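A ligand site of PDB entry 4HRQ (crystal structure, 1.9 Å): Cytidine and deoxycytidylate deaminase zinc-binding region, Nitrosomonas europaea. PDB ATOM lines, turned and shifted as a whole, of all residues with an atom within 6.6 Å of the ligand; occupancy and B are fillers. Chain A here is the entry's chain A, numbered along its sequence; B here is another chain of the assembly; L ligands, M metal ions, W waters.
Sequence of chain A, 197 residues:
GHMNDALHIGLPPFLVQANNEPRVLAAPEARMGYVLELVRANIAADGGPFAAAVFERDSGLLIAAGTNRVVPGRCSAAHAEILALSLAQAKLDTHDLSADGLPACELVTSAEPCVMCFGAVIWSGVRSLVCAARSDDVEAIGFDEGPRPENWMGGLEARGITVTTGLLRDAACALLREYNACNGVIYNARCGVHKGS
Water W2 lies within hydrogen-bond range of the side-chain carboxylate (OE2) of Glu 81 (2.5 Å), a nitrogen (N1) of the ligand (2.7 Å) and the backbone NH (N) of Cys 114 (2.9 Å).
Water W3 bridges N1 of the ligand and O of Glu 112.
The backbone NH of Ala 80 sits at hydrogen-bond distance from a nitrogen (N5) of the ligand (3.0 Å).
OE1 of Glu 145 is in hydrogen-bond range of N2 of the ligand (2.9 Å).
The backbone carbonyl oxygen (O) of Asp 144 lies within hydrogen-bond range of a nitrogen (N2) of the ligand (3.2 Å).
OE1 of Glu 81 lies close to N6 of the ligand, 2.9 Å away.
OD1 of Asn 68 lies within hydrogen-bond range of N4 of the ligand, 2.8 Å away.
CB of Phe 50 touches N5 of the ligand (3.5 Å).
CB of His 79 touches N5 of the ligand, 3.3 Å away.
Cys 114 touches the ligand.
Hydrophobic or aromatic side chains that line the ligand: Phe 50, His 79 and Ala 80.
Of the 25 residues printed, 8 come within 4 Å of the ligand.
N of Val 70 lies close to ND2 of Asn 68, at 2.9 Å.
The backbone NH (N) of Gly 146 lies within hydrogen-bond range of the side-chain carboxylate (OD1) of Asp 144, 2.9 Å away.
SG of Cys 117 sits close to OE1 of Glu 81 (3.6 Å).
N of Asn 68 sits at hydrogen-bond distance from O of Phe 50, at 3.3 Å.
O of Asn 68 sits at hydrogen-bond distance from N of Gly 48 (3.3 Å).
N of Cys 114 lies close to OE1 of Glu 145, 3.4 Å away.
OE2 of Glu 145 lies close to O of Glu 112 (2.6 Å).
The side-chain sulfur of Cys 114 lies close to the indole nitrogen of Trp 123 of chain B, 3.5 Å away.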
ATOM      1  N   GLY A  48       3.907  -9.946  -4.055  1.00  0.00           N
ATOM      2  CA  GLY A  48       3.682  -8.732  -4.825  1.00  0.00           C
ATOM      3  C   GLY A  48       2.432  -8.799  -5.680  1.00  0.00           C
ATOM      4  O   GLY A  48       1.903  -9.882  -5.912  1.00  0.00           O
ATOM      5  N   PRO A  49       1.929  -7.647  -6.181  1.00  0.00           N
ATOM      6  CA  PRO A  49       0.726  -7.597  -7.012  1.00  0.00           C
ATOM      7  C   PRO A  49       0.958  -7.979  -8.477  1.00  0.00           C
ATOM      8  O   PRO A  49       0.576  -7.234  -9.374  1.00  0.00           O
ATOM      9  CB  PRO A  49       0.274  -6.155  -6.864  1.00  0.00           C
ATOM     10  CG  PRO A  49       1.576  -5.434  -6.835  1.00  0.00           C
ATOM     11  CD  PRO A  49       2.416  -6.292  -5.907  1.00  0.00           C
ATOM     12  N   PHE A  50       1.559  -9.142  -8.697  1.00  0.00           N
ATOM     13  CA  PHE A  50       1.861  -9.605 -10.037  1.00  0.00           C
ATOM     14  C   PHE A  50       1.677 -11.108 -10.174  1.00  0.00           C
ATOM     15  O   PHE A  50       1.904 -11.868  -9.235  1.00  0.00           O
ATOM     16  CB  PHE A  50       3.309  -9.273 -10.387  1.00  0.00           C
ATOM     17  CG  PHE A  50       3.622  -7.819 -10.345  1.00  0.00           C
ATOM     18  CD1 PHE A  50       3.408  -7.012 -11.452  1.00  0.00           C
ATOM     19  CD2 PHE A  50       4.162  -7.257  -9.195  1.00  0.00           C
ATOM     20  CE1 PHE A  50       3.728  -5.663 -11.418  1.00  0.00           C
ATOM     21  CE2 PHE A  50       4.493  -5.910  -9.152  1.00  0.00           C
ATOM     22  CZ  PHE A  50       4.277  -5.112 -10.258  1.00  0.00           C
ATOM     23  N   ALA A  51       1.268 -11.528 -11.369  1.00  0.00           N
ATOM     24  CA  ALA A  51       1.078 -12.934 -11.638  1.00  0.00           C
ATOM     25  C   ALA A  51       1.199 -13.155 -13.144  1.00  0.00           C
ATOM     26  O   ALA A  51       1.046 -12.225 -13.927  1.00  0.00           O
ATOM     27  CB  ALA A  51      -0.286 -13.387 -11.128  1.00  0.00           C
ATOM     28  N   THR A  67       3.823 -16.280  -9.525  1.00  0.00           N
ATOM     29  CA  THR A  67       3.502 -14.983  -8.936  1.00  0.00           C
ATOM     30  C   THR A  67       4.759 -14.410  -8.291  1.00  0.00           C
ATOM     31  O   THR A  67       5.756 -15.099  -8.109  1.00  0.00           O
ATOM     32  CB  THR A  67       2.397 -15.109  -7.866  1.00  0.00           C
ATOM     33  OG1 THR A  67       2.904 -15.842  -6.747  1.00  0.00           O
ATOM     34  CG2 THR A  67       1.193 -15.837  -8.426  1.00  0.00           C
ATOM     35  N   ASN A  68       4.690 -13.134  -7.929  1.00  0.00           N
ATOM     36  CA  ASN A  68       5.815 -12.454  -7.308  1.00  0.00           C
ATOM     37  C   ASN A  68       5.986 -12.997  -5.906  1.00  0.00           C
ATOM     38  O   ASN A  68       5.082 -12.897  -5.078  1.00  0.00           O
ATOM     39  CB  ASN A  68       5.537 -10.939  -7.272  1.00  0.00           C
ATOM     40  CG  ASN A  68       6.654 -10.160  -6.612  1.00  0.00           C
ATOM     41  OD1 ASN A  68       7.130  -9.165  -7.153  1.00  0.00           O
ATOM     42  ND2 ASN A  68       7.074 -10.598  -5.430  1.00  0.00           N
ATOM     43  N   ARG A  69       7.137 -13.606  -5.653  1.00  0.00           N
ATOM     44  CA  ARG A  69       7.435 -14.157  -4.338  1.00  0.00           C
ATOM     45  C   ARG A  69       8.773 -13.601  -3.859  1.00  0.00           C
ATOM     46  O   ARG A  69       9.495 -14.261  -3.107  1.00  0.00           O
ATOM     47  CB  ARG A  69       7.495 -15.681  -4.409  1.00  0.00           C
ATOM     48  CG  ARG A  69       6.247 -16.378  -4.959  1.00  0.00           C
ATOM     49  CD  ARG A  69       4.976 -16.015  -4.197  1.00  0.00           C
ATOM     50  NE  ARG A  69       5.080 -16.304  -2.768  1.00  0.00           N
ATOM     51  CZ  ARG A  69       4.165 -15.935  -1.869  1.00  0.00           C
ATOM     52  NH1 ARG A  69       3.093 -15.268  -2.256  1.00  0.00           N
ATOM     53  NH2 ARG A  69       4.327 -16.257  -0.592  1.00  0.00           N
ATOM     54  N   VAL A  70       9.095 -12.387  -4.304  1.00  0.00           N
ATOM     55  CA  VAL A  70      10.358 -11.728  -3.942  1.00  0.00           C
ATOM     56  C   VAL A  70      10.630 -11.631  -2.439  1.00  0.00           C
ATOM     57  O   VAL A  70      11.650 -12.131  -1.957  1.00  0.00           O
ATOM     58  CB  VAL A  70      10.428 -10.311  -4.575  1.00  0.00           C
ATOM     59  CG1 VAL A  70      11.562  -9.498  -3.949  1.00  0.00           C
ATOM     60  CG2 VAL A  70      10.635 -10.417  -6.090  1.00  0.00           C
ATOM     61  N   ALA A  78      12.649 -13.529  -8.201  1.00  0.00           N
ATOM     62  CA  ALA A  78      11.371 -14.241  -8.203  1.00  0.00           C
ATOM     63  C   ALA A  78      10.164 -13.422  -8.668  1.00  0.00           C
ATOM     64  O   ALA A  78       9.188 -13.256  -7.923  1.00  0.00           O
ATOM     65  CB  ALA A  78      11.102 -14.829  -6.815  1.00  0.00           C
ATOM     66  N   HIS A  79      10.229 -12.915  -9.891  1.00  0.00           N
ATOM     67  CA  HIS A  79       9.107 -12.157 -10.456  1.00  0.00           C
ATOM     68  C   HIS A  79       8.128 -13.163 -11.049  1.00  0.00           C
ATOM     69  O   HIS A  79       8.496 -14.304 -11.316  1.00  0.00           O
ATOM     70  CB  HIS A  79       9.592 -11.194 -11.539  1.00  0.00           C
ATOM     71  CG  HIS A  79      10.285  -9.981 -11.000  1.00  0.00           C
ATOM     72  ND1 HIS A  79      10.458  -8.827 -11.750  1.00  0.00           N
ATOM     73  CD2 HIS A  79      10.824  -9.721  -9.796  1.00  0.00           C
ATOM     74  CE1 HIS A  79      11.065  -7.912 -11.020  1.00  0.00           C
ATOM     75  NE2 HIS A  79      11.295  -8.423  -9.826  1.00  0.00           N
ATOM     76  N   ALA A  80       6.877 -12.751 -11.232  1.00  0.00           N
ATOM     77  CA  ALA A  80       5.830 -13.605 -11.798  1.00  0.00           C
ATOM     78  C   ALA A  80       6.308 -14.375 -13.003  1.00  0.00           C
ATOM     79  O   ALA A  80       6.247 -15.605 -13.059  1.00  0.00           O
ATOM     80  CB  ALA A  80       4.629 -12.769 -12.205  1.00  0.00           C
ATOM     81  N   GLU A  81       6.765 -13.610 -13.991  1.00  0.00           N
ATOM     82  CA  GLU A  81       7.231 -14.139 -15.254  1.00  0.00           C
ATOM     83  C   GLU A  81       8.310 -15.199 -15.105  1.00  0.00           C
ATOM     84  O   GLU A  81       8.264 -16.233 -15.770  1.00  0.00           O
ATOM     85  CB  GLU A  81       7.742 -13.000 -16.137  1.00  0.00           C
ATOM     86  CG  GLU A  81       6.733 -11.882 -16.357  1.00  0.00           C
ATOM     87  CD  GLU A  81       6.915 -10.704 -15.396  1.00  0.00           C
ATOM     88  OE1 GLU A  81       6.907 -10.904 -14.171  1.00  0.00           O
ATOM     89  OE2 GLU A  81       7.085  -9.568 -15.891  1.00  0.00           O
ATOM     90  N   THR A 109       0.714 -12.253 -18.724  1.00  0.00           N
ATOM     91  CA  THR A 109       1.193 -11.551 -17.546  1.00  0.00           C
ATOM     92  C   THR A 109       0.307 -10.368 -17.147  1.00  0.00           C
ATOM     93  O   THR A 109      -0.233  -9.655 -17.999  1.00  0.00           O
ATOM     94  CB  THR A 109       2.642 -11.092 -17.790  1.00  0.00           C
ATOM     95  OG1 THR A 109       3.118 -10.345 -16.668  1.00  0.00           O
ATOM     96  CG2 THR A 109       2.709 -10.229 -19.044  1.00  0.00           C
ATOM     97  N   SER A 110       0.166 -10.149 -15.841  1.00  0.00           N
ATOM     98  CA  SER A 110      -0.665  -9.080 -15.291  1.00  0.00           C
ATOM     99  C   SER A 110      -0.142  -7.673 -15.590  1.00  0.00           C
ATOM    100  O   SER A 110      -0.868  -6.698 -15.430  1.00  0.00           O
ATOM    101  CB  SER A 110      -0.810  -9.256 -13.778  1.00  0.00           C
ATOM    102  OG  SER A 110       0.450  -9.147 -13.140  1.00  0.00           O
ATOM    103  N   ALA A 111       1.117  -7.587 -16.000  1.00  0.00           N
ATOM    104  CA  ALA A 111       1.729  -6.292 -16.302  1.00  0.00           C
ATOM    105  C   ALA A 111       2.900  -6.455 -17.272  1.00  0.00           C
ATOM    106  O   ALA A 111       3.517  -7.528 -17.323  1.00  0.00           O
ATOM    107  CB  ALA A 111       2.223  -5.640 -15.009  1.00  0.00           C
ATOM    108  N   GLU A 112       3.205  -5.401 -18.020  1.00  0.00           N
ATOM    109  CA  GLU A 112       4.317  -5.457 -18.969  1.00  0.00           C
ATOM    110  C   GLU A 112       5.592  -5.786 -18.191  1.00  0.00           C
ATOM    111  O   GLU A 112       5.807  -5.296 -17.082  1.00  0.00           O
ATOM    112  CB  GLU A 112       4.449  -4.117 -19.697  1.00  0.00           C
ATOM    113  CG  GLU A 112       3.227  -3.810 -20.566  1.00  0.00           C
ATOM    114  CD  GLU A 112       3.342  -2.492 -21.332  1.00  0.00           C
ATOM    115  OE1 GLU A 112       4.201  -1.665 -20.961  1.00  0.00           O
ATOM    116  OE2 GLU A 112       2.554  -2.296 -22.278  1.00  0.00           O
ATOM    117  N   PRO A 113       6.445  -6.655 -18.756  1.00  0.00           N
ATOM    118  CA  PRO A 113       7.692  -7.080 -18.127  1.00  0.00           C
ATOM    119  C   PRO A 113       8.767  -6.041 -17.837  1.00  0.00           C
ATOM    120  O   PRO A 113       8.959  -5.087 -18.585  1.00  0.00           O
ATOM    121  CB  PRO A 113       8.186  -8.162 -19.086  1.00  0.00           C
ATOM    122  CG  PRO A 113       7.760  -7.628 -20.419  1.00  0.00           C
ATOM    123  CD  PRO A 113       6.333  -7.181 -20.130  1.00  0.00           C
ATOM    124  N   CYS A 114       9.472  -6.229 -16.723  1.00  0.00           N
ATOM    125  CA  CYS A 114      10.558  -5.346 -16.345  1.00  0.00           C
ATOM    126  C   CYS A 114      11.704  -5.784 -17.252  1.00  0.00           C
ATOM    127  O   CYS A 114      11.581  -6.787 -17.955  1.00  0.00           O
ATOM    128  CB  CYS A 114      10.959  -5.548 -14.877  1.00  0.00           C
ATOM    129  SG  CYS A 114      11.909  -7.062 -14.546  1.00  0.00           S
ATOM    130  N   CYS A 117      12.730  -9.601 -16.772  1.00  0.00           N
ATOM    131  CA  CYS A 117      11.796 -10.544 -17.366  1.00  0.00           C
ATOM    132  C   CYS A 117      11.723 -10.426 -18.877  1.00  0.00           C
ATOM    133  O   CYS A 117      11.375 -11.381 -19.571  1.00  0.00           O
ATOM    134  CB  CYS A 117      10.427 -10.381 -16.715  1.00  0.00           C
ATOM    135  SG  CYS A 117      10.467 -10.798 -14.944  1.00  0.00           S
ATOM    136  N   VAL A 138       2.238   0.420 -13.670  1.00  0.00           N
ATOM    137  CA  VAL A 138       3.086  -0.225 -12.676  1.00  0.00           C
ATOM    138  C   VAL A 138       4.005   0.766 -11.976  1.00  0.00           C
ATOM    139  O   VAL A 138       4.138   0.752 -10.752  1.00  0.00           O
ATOM    140  CB  VAL A 138       3.959  -1.318 -13.347  1.00  0.00           C
ATOM    141  CG1 VAL A 138       4.756  -2.068 -12.296  1.00  0.00           C
ATOM    142  CG2 VAL A 138       3.073  -2.284 -14.123  1.00  0.00           C
ATOM    143  N   PHE A 143       6.506   0.885  -8.782  1.00  0.00           N
ATOM    144  CA  PHE A 143       7.236  -0.308  -9.189  1.00  0.00           C
ATOM    145  C   PHE A 143       8.045  -0.042 -10.446  1.00  0.00           C
ATOM    146  O   PHE A 143       7.509   0.209 -11.518  1.00  0.00           O
ATOM    147  CB  PHE A 143       6.262  -1.464  -9.423  1.00  0.00           C
ATOM    148  CG  PHE A 143       5.537  -1.903  -8.182  1.00  0.00           C
ATOM    149  CD1 PHE A 143       6.111  -1.727  -6.930  1.00  0.00           C
ATOM    150  CD2 PHE A 143       4.303  -2.533  -8.266  1.00  0.00           C
ATOM    151  CE1 PHE A 143       5.470  -2.186  -5.784  1.00  0.00           C
ATOM    152  CE2 PHE A 143       3.661  -2.993  -7.130  1.00  0.00           C
ATOM    153  CZ  PHE A 143       4.246  -2.819  -5.878  1.00  0.00           C
ATOM    154  N   ASP A 144       9.373  -0.091 -10.280  1.00  0.00           N
ATOM    155  CA  ASP A 144      10.302   0.171 -11.373  1.00  0.00           C
ATOM    156  C   ASP A 144      10.291  -0.959 -12.403  1.00  0.00           C
ATOM    157  O   ASP A 144      10.270  -2.134 -12.044  1.00  0.00           O
ATOM    158  CB  ASP A 144      11.715   0.292 -10.789  1.00  0.00           C
ATOM    159  CG  ASP A 144      12.611   1.205 -11.602  1.00  0.00           C
ATOM    160  OD1 ASP A 144      12.391   1.339 -12.823  1.00  0.00           O
ATOM    161  OD2 ASP A 144      13.548   1.775 -11.016  1.00  0.00           O
ATOM    162  N   GLU A 145      10.312  -0.595 -13.687  1.00  0.00           N
ATOM    163  CA  GLU A 145      10.347  -1.595 -14.755  1.00  0.00           C
ATOM    164  C   GLU A 145      11.797  -1.758 -15.190  1.00  0.00           C
ATOM    165  O   GLU A 145      12.161  -2.743 -15.848  1.00  0.00           O
ATOM    166  CB  GLU A 145       9.487  -1.157 -15.937  1.00  0.00           C
ATOM    167  CG  GLU A 145       7.978  -1.232 -15.682  1.00  0.00           C
ATOM    168  CD  GLU A 145       7.416  -2.641 -15.774  1.00  0.00           C
ATOM    169  OE1 GLU A 145       8.019  -3.578 -15.203  1.00  0.00           O
ATOM    170  OE2 GLU A 145       6.367  -2.816 -16.428  1.00  0.00           O
ATOM    171  N   GLY A 146      12.636  -0.785 -14.835  1.00  0.00           N
ATOM    172  CA  GLY A 146      14.035  -0.865 -15.195  1.00  0.00           C
ATOM    173  C   GLY A 146      14.330  -0.302 -16.572  1.00  0.00           C
ATOM    174  O   GLY A 146      13.415   0.070 -17.318  1.00  0.00           O
ATOM    175  N   TRP B 123      18.057  -5.233  -9.622  1.00  0.00           N
ATOM    176  CA  TRP B 123      17.127  -5.504  -8.517  1.00  0.00           C
ATOM    177  C   TRP B 123      17.748  -6.242  -7.335  1.00  0.00           C
ATOM    178  O   TRP B 123      17.130  -6.337  -6.283  1.00  0.00           O
ATOM    179  CB  TRP B 123      15.932  -6.346  -8.994  1.00  0.00           C
ATOM    180  CG  TRP B 123      15.266  -5.897 -10.251  1.00  0.00           C
ATOM    181  CD1 TRP B 123      14.876  -6.692 -11.292  1.00  0.00           C
ATOM    182  CD2 TRP B 123      14.893  -4.557 -10.601  1.00  0.00           C
ATOM    183  NE1 TRP B 123      14.279  -5.932 -12.267  1.00  0.00           N
ATOM    184  CE2 TRP B 123      14.281  -4.615 -11.874  1.00  0.00           C
ATOM    185  CE3 TRP B 123      15.025  -3.308  -9.967  1.00  0.00           C
ATOM    186  CZ2 TRP B 123      13.800  -3.477 -12.527  1.00  0.00           C
ATOM    187  CZ3 TRP B 123      14.541  -2.179 -10.619  1.00  0.00           C
ATOM    188  CH2 TRP B 123      13.933  -2.269 -11.888  1.00  0.00           C
HETATM  189  C1  LIG L   1       7.178  -7.883 -11.562  1.00  0.00           C
HETATM  190  N1  LIG L   1       7.410  -6.733 -12.326  1.00  0.00           N
HETATM  191  C2  LIG L   1       7.877  -5.582 -11.754  1.00  0.00           C
HETATM  192  N2  LIG L   1       8.107  -4.499 -12.480  1.00  0.00           N
HETATM  193  N3  LIG L   1       8.114  -5.581 -10.328  1.00  0.00           N
HETATM  194  C3  LIG L   1       7.856  -6.799  -9.574  1.00  0.00           C
HETATM  195  O1  LIG L   1       8.071  -6.767  -8.351  1.00  0.00           O
HETATM  196  C4  LIG L   1       7.391  -7.930 -10.229  1.00  0.00           C
HETATM  197  N4  LIG L   1       7.034  -9.183  -9.908  1.00  0.00           N
HETATM  198  N5  LIG L   1       6.690  -9.781 -10.865  1.00  0.00           N
HETATM  199  N6  LIG L   1       6.736  -9.125 -11.842  1.00  0.00           N
HETATM  200 ZN    ZN M   1      10.288  -8.691 -13.913  1.00  0.00          ZN
HETATM  201  O   HOH W   1       7.113  -4.328  -7.113  1.00  0.00           O
HETATM  202  O   HOH W   2       8.379  -7.807 -14.610  1.00  0.00           O
HETATM  203  O   HOH W   3       5.470  -6.367 -14.211  1.00  0.00           O
